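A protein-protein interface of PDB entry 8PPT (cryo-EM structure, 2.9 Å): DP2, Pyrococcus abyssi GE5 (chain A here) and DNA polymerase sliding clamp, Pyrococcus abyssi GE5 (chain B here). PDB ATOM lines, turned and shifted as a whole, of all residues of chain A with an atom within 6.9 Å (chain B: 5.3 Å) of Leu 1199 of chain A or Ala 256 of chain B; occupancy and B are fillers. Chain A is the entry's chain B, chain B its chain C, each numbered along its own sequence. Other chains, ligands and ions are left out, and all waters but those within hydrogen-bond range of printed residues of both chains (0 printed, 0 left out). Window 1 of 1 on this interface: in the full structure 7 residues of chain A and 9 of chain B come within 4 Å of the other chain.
N of Leu 1201 of chain A sits at hydrogen-bond distance from O of Arg 57 of chain B, 3.0 Å away.
N of Leu 1199 of chain A lies within hydrogen-bond range of O of Pro 257 of chain B (3.3 Å).
The backbone carbonyl oxygen (O) of Thr 1197 of chain A sits at hydrogen-bond distance from the backbone NH (N) of Val 259 of chain B.
The side-chain hydroxyl (OG1) of Thr 1200 of chain A sits close to the backbone carbonyl oxygen (O) of Arg 57 of chain B, 2.4 Å away.
The backbone NH (N) of Ala 256 of chain B is in hydrogen-bond range of the backbone carbonyl oxygen (O) of Val 58 of chain B.
The backbone carbonyl oxygen of Ala 210 of chain B sits at hydrogen-bond distance from the backbone NH of Arg 258 of chain B, at 3.0 Å.
Of the 11 printed residues of chain B, 7 touch a printed residue of chain A.
Printed residues of chain B that touch a printed residue of chain A: Arg 57, Val 58, Leu 254, Ala 256, Pro 257, Arg 258 and Val 259.
Of the 6 printed residues of chain A, 5 touch a printed residue of chain B.
Printed residues of chain A that touch a printed residue of chain B: Thr 1197, Gln 1198, Leu 1199, Thr 1200 and Leu 1201.
Hydrophobic or aromatic side chains of chain A that line the printed part of chain B: Leu 1199 and Leu 1201.
Along chain A the printed residues that touch a printed residue of chain B span positions 1197 to 1201.
Printed residues of chain B within 4 Å of Thr 1197 of chain A: Arg 258 and Val 259.
Of the printed residues of chain B, Gln 1198 of chain A touches Val 58 (3.2 Å), Ala 256 (3.6 Å), Pro 257 (3.8 Å) and Arg 258 (3.3 Å).
Leu 1199 of chain A touches just these residues of chain B: Val 58, Ala 256, Pro 257 and Val 259.
Ala 210 of chain B touches none of the printed residues of chain A.
Tyr 211 of chain B touches none of the printed residues of chain A.
Of the printed residues of chain A, Leu 254 of chain B touches Leu 1201 (3.7 Å).
Of chain A, only Gln 1198 (3.6 Å), Leu 1199 (3.97 Å) and Leu 1201 (3.6 Å) come within 4 Å of Ala 256 of chain B.
The nearest residue of chain B that does not touch Leu 1199 of chain A is Arg 258 of chain B (4.1 Å).
Among the printed residues, pairs that only touch across the chains: Thr 1197 of chain A with Arg 258 of chain B (3.4 Å), Gln 1198 of chain A with Val 58 of chain B (3.2 Å), Gln 1198 of chain A with Ala 256 of chain B (3.6 Å), Gln 1198 of chain A with Pro 257 of chain B (3.8 Å), Gln 1198 of chain A with Arg 258 of chain B (3.3 Å), Leu 1199 of chain A with Val 58 of chain B (3.9 Å), Leu 1199 of chain A with Ala 256 of chain B (3.97 Å), Leu 1199 of chain A with Val 259 of chain B (3.7 Å), Leu 1201 of chain A with Val 58 of chain B (3.2 Å), Leu 1201 of chain A with Leu 254 of chain B (3.7 Å) and Leu 1201 of chain A with Ala 256 of chain B (3.6 Å).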
ATOM      1  N   GLU A1196     -16.594  22.577 -31.453  1.00  0.00           N
ATOM      2  CA  GLU A1196     -17.877  23.098 -30.984  1.00  0.00           C
ATOM      3  C   GLU A1196     -18.111  22.603 -29.561  1.00  0.00           C
ATOM      4  O   GLU A1196     -18.480  21.447 -29.336  1.00  0.00           O
ATOM      5  CB  GLU A1196     -18.999  22.692 -31.936  1.00  0.00           C
ATOM      6  CG  GLU A1196     -19.090  21.205 -32.249  1.00  0.00           C
ATOM      7  CD  GLU A1196     -18.613  20.870 -33.650  1.00  0.00           C
ATOM      8  OE1 GLU A1196     -19.458  20.803 -34.566  1.00  0.00           O
ATOM      9  OE2 GLU A1196     -17.393  20.672 -33.834  1.00  0.00           O
ATOM     10  N   THR A1197     -17.878  23.480 -28.587  1.00  0.00           N
ATOM     11  CA  THR A1197     -17.982  23.132 -27.177  1.00  0.00           C
ATOM     12  C   THR A1197     -19.137  23.834 -26.476  1.00  0.00           C
ATOM     13  O   THR A1197     -19.240  23.755 -25.248  1.00  0.00           O
ATOM     14  CB  THR A1197     -16.670  23.455 -26.457  1.00  0.00           C
ATOM     15  OG1 THR A1197     -16.106  24.656 -26.999  1.00  0.00           O
ATOM     16  CG2 THR A1197     -15.677  22.315 -26.624  1.00  0.00           C
ATOM     17  N   GLN A1198     -20.006  24.515 -27.217  1.00  0.00           N
ATOM     18  CA  GLN A1198     -21.111  25.260 -26.629  1.00  0.00           C
ATOM     19  C   GLN A1198     -22.405  24.866 -27.324  1.00  0.00           C
ATOM     20  O   GLN A1198     -22.479  24.880 -28.557  1.00  0.00           O
ATOM     21  CB  GLN A1198     -20.882  26.769 -26.750  1.00  0.00           C
ATOM     22  CG  GLN A1198     -22.105  27.601 -26.434  1.00  0.00           C
ATOM     23  CD  GLN A1198     -22.277  27.813 -24.945  1.00  0.00           C
ATOM     24  OE1 GLN A1198     -21.318  27.723 -24.181  1.00  0.00           O
ATOM     25  NE2 GLN A1198     -23.503  28.078 -24.524  1.00  0.00           N
ATOM     26  N   LEU A1199     -23.419  24.521 -26.536  1.00  0.00           N
ATOM     27  CA  LEU A1199     -24.717  24.142 -27.071  1.00  0.00           C
ATOM     28  C   LEU A1199     -25.574  25.392 -27.270  1.00  0.00           C
ATOM     29  O   LEU A1199     -25.097  26.524 -27.158  1.00  0.00           O
ATOM     30  CB  LEU A1199     -25.395  23.129 -26.150  1.00  0.00           C
ATOM     31  CG  LEU A1199     -24.601  21.872 -25.795  1.00  0.00           C
ATOM     32  CD1 LEU A1199     -25.499  20.850 -25.122  1.00  0.00           C
ATOM     33  CD2 LEU A1199     -23.955  21.279 -27.036  1.00  0.00           C
ATOM     34  N   THR A1200     -26.856  25.197 -27.573  1.00  0.00           N
ATOM     35  CA  THR A1200     -27.765  26.314 -27.782  1.00  0.00           C
ATOM     36  C   THR A1200     -29.161  25.914 -27.334  1.00  0.00           C
ATOM     37  O   THR A1200     -29.510  24.730 -27.296  1.00  0.00           O
ATOM     38  CB  THR A1200     -27.787  26.762 -29.248  1.00  0.00           C
ATOM     39  OG1 THR A1200     -28.921  27.609 -29.471  1.00  0.00           O
ATOM     40  CG2 THR A1200     -27.870  25.556 -30.169  1.00  0.00           C
ATOM     41  N   LEU A1201     -29.961  26.925 -26.990  1.00  0.00           N
ATOM     42  CA  LEU A1201     -31.320  26.671 -26.526  1.00  0.00           C
ATOM     43  C   LEU A1201     -32.222  26.202 -27.662  1.00  0.00           C
ATOM     44  O   LEU A1201     -32.950  25.214 -27.516  1.00  0.00           O
ATOM     45  CB  LEU A1201     -31.890  27.932 -25.878  1.00  0.00           C
ATOM     46  CG  LEU A1201     -31.970  27.956 -24.353  1.00  0.00           C
ATOM     47  CD1 LEU A1201     -30.585  28.012 -23.747  1.00  0.00           C
ATOM     48  CD2 LEU A1201     -32.795  29.146 -23.900  1.00  0.00           C
ATOM     49  N   ARG B  57     -28.682  32.687 -29.689  1.00  0.00           N
ATOM     50  CA  ARG B  57     -29.648  31.676 -29.256  1.00  0.00           C
ATOM     51  C   ARG B  57     -29.075  30.812 -28.133  1.00  0.00           C
ATOM     52  O   ARG B  57     -29.171  29.583 -28.153  1.00  0.00           O
ATOM     53  CB  ARG B  57     -30.111  30.813 -30.432  1.00  0.00           C
ATOM     54  CG  ARG B  57     -30.409  31.595 -31.700  1.00  0.00           C
ATOM     55  CD  ARG B  57     -30.762  30.669 -32.852  1.00  0.00           C
ATOM     56  NE  ARG B  57     -30.191  29.340 -32.678  1.00  0.00           N
ATOM     57  CZ  ARG B  57     -29.178  28.860 -33.388  1.00  0.00           C
ATOM     58  NH1 ARG B  57     -28.595  29.580 -34.331  1.00  0.00           N
ATOM     59  NH2 ARG B  57     -28.742  27.627 -33.145  1.00  0.00           N
ATOM     60  N   VAL B  58     -28.474  31.470 -27.144  1.00  0.00           N
ATOM     61  CA  VAL B  58     -27.835  30.771 -26.035  1.00  0.00           C
ATOM     62  C   VAL B  58     -28.422  31.237 -24.707  1.00  0.00           C
ATOM     63  O   VAL B  58     -28.477  30.472 -23.738  1.00  0.00           O
ATOM     64  CB  VAL B  58     -26.309  30.981 -26.070  1.00  0.00           C
ATOM     65  CG1 VAL B  58     -25.655  30.413 -24.828  1.00  0.00           C
ATOM     66  CG2 VAL B  58     -25.715  30.350 -27.318  1.00  0.00           C
ATOM     67  N   ALA B 210     -21.436  22.664 -16.728  1.00  0.00           N
ATOM     68  CA  ALA B 210     -20.389  23.619 -17.064  1.00  0.00           C
ATOM     69  C   ALA B 210     -20.988  24.730 -17.910  1.00  0.00           C
ATOM     70  O   ALA B 210     -21.823  24.471 -18.779  1.00  0.00           O
ATOM     71  CB  ALA B 210     -19.232  22.946 -17.808  1.00  0.00           C
ATOM     72  N   TYR B 211     -20.559  25.966 -17.653  1.00  0.00           N
ATOM     73  CA  TYR B 211     -21.114  27.131 -18.325  1.00  0.00           C
ATOM     74  C   TYR B 211     -20.002  28.103 -18.687  1.00  0.00           C
ATOM     75  O   TYR B 211     -18.982  28.190 -18.000  1.00  0.00           O
ATOM     76  CB  TYR B 211     -22.165  27.830 -17.454  1.00  0.00           C
ATOM     77  CG  TYR B 211     -23.254  26.896 -16.982  1.00  0.00           C
ATOM     78  CD1 TYR B 211     -23.144  26.232 -15.771  1.00  0.00           C
ATOM     79  CD2 TYR B 211     -24.379  26.663 -17.757  1.00  0.00           C
ATOM     80  CE1 TYR B 211     -24.127  25.372 -15.338  1.00  0.00           C
ATOM     81  CE2 TYR B 211     -25.369  25.803 -17.333  1.00  0.00           C
ATOM     82  CZ  TYR B 211     -25.237  25.160 -16.123  1.00  0.00           C
ATOM     83  OH  TYR B 211     -26.220  24.301 -15.693  1.00  0.00           O
ATOM     84  N   PRO B 238     -29.917  23.184 -19.176  1.00  0.00           N
ATOM     85  CA  PRO B 238     -29.761  24.621 -18.898  1.00  0.00           C
ATOM     86  C   PRO B 238     -29.926  25.003 -17.435  1.00  0.00           C
ATOM     87  O   PRO B 238     -30.467  24.238 -16.631  1.00  0.00           O
ATOM     88  CB  PRO B 238     -30.856  25.260 -19.760  1.00  0.00           C
ATOM     89  CG  PRO B 238     -31.051  24.310 -20.877  1.00  0.00           C
ATOM     90  CD  PRO B 238     -30.825  22.940 -20.311  1.00  0.00           C
ATOM     91  N   LEU B 254     -31.691  32.211 -18.510  1.00  0.00           N
ATOM     92  CA  LEU B 254     -31.584  30.827 -18.956  1.00  0.00           C
ATOM     93  C   LEU B 254     -30.344  30.702 -19.827  1.00  0.00           C
ATOM     94  O   LEU B 254     -30.228  31.390 -20.845  1.00  0.00           O
ATOM     95  CB  LEU B 254     -32.836  30.397 -19.722  1.00  0.00           C
ATOM     96  CG  LEU B 254     -33.173  28.905 -19.706  1.00  0.00           C
ATOM     97  CD1 LEU B 254     -33.456  28.434 -18.290  1.00  0.00           C
ATOM     98  CD2 LEU B 254     -34.356  28.618 -20.613  1.00  0.00           C
ATOM     99  N   LEU B 255     -29.426  29.826 -19.431  1.00  0.00           N
ATOM    100  CA  LEU B 255     -28.144  29.674 -20.105  1.00  0.00           C
ATOM    101  C   LEU B 255     -27.936  28.223 -20.517  1.00  0.00           C
ATOM    102  O   LEU B 255     -28.117  27.311 -19.705  1.00  0.00           O
ATOM    103  CB  LEU B 255     -26.997  30.139 -19.202  1.00  0.00           C
ATOM    104  CG  LEU B 255     -25.620  30.238 -19.854  1.00  0.00           C
ATOM    105  CD1 LEU B 255     -25.589  31.396 -20.823  1.00  0.00           C
ATOM    106  CD2 LEU B 255     -24.548  30.399 -18.797  1.00  0.00           C
ATOM    107  N   ALA B 256     -27.556  28.018 -21.776  1.00  0.00           N
ATOM    108  CA  ALA B 256     -27.238  26.691 -22.268  1.00  0.00           C
ATOM    109  C   ALA B 256     -25.902  26.220 -21.698  1.00  0.00           C
ATOM    110  O   ALA B 256     -25.006  27.026 -21.440  1.00  0.00           O
ATOM    111  CB  ALA B 256     -27.188  26.690 -23.793  1.00  0.00           C
ATOM    112  N   PRO B 257     -25.743  24.917 -21.496  1.00  0.00           N
ATOM    113  CA  PRO B 257     -24.493  24.390 -20.943  1.00  0.00           C
ATOM    114  C   PRO B 257     -23.452  24.183 -22.039  1.00  0.00           C
ATOM    115  O   PRO B 257     -23.662  24.507 -23.206  1.00  0.00           O
ATOM    116  CB  PRO B 257     -24.917  23.061 -20.307  1.00  0.00           C
ATOM    117  CG  PRO B 257     -26.296  22.759 -20.838  1.00  0.00           C
ATOM    118  CD  PRO B 257     -26.715  23.848 -21.771  1.00  0.00           C
ATOM    119  N   ARG B 258     -22.311  23.633 -21.636  1.00  0.00           N
ATOM    120  CA  ARG B 258     -21.193  23.381 -22.528  1.00  0.00           C
ATOM    121  C   ARG B 258     -21.160  21.904 -22.916  1.00  0.00           C
ATOM    122  O   ARG B 258     -22.090  21.142 -22.629  1.00  0.00           O
ATOM    123  CB  ARG B 258     -19.885  23.823 -21.868  1.00  0.00           C
ATOM    124  CG  ARG B 258     -19.924  25.230 -21.300  1.00  0.00           C
ATOM    125  CD  ARG B 258     -19.167  26.208 -22.178  1.00  0.00           C
ATOM    126  NE  ARG B 258     -17.757  25.864 -22.298  1.00  0.00           N
ATOM    127  CZ  ARG B 258     -16.854  26.621 -22.904  1.00  0.00           C
ATOM    128  NH1 ARG B 258     -17.182  27.775 -23.462  1.00  0.00           N
ATOM    129  NH2 ARG B 258     -15.590  26.211 -22.953  1.00  0.00           N
ATOM    130  N   VAL B 259     -20.084  21.499 -23.587  1.00  0.00           N
ATOM    131  CA  VAL B 259     -19.880  20.120 -24.026  1.00  0.00           C
ATOM    132  C   VAL B 259     -20.989  19.686 -24.975  1.00  0.00           C
ATOM    133  O   VAL B 259     -20.773  19.569 -26.180  1.00  0.00           O
ATOM    134  CB  VAL B 259     -19.777  19.155 -22.827  1.00  0.00           C
ATOM    135  CG1 VAL B 259     -20.090  17.730 -23.258  1.00  0.00           C
ATOM    136  CG2 VAL B 259     -18.395  19.238 -22.197  1.00  0.00           C
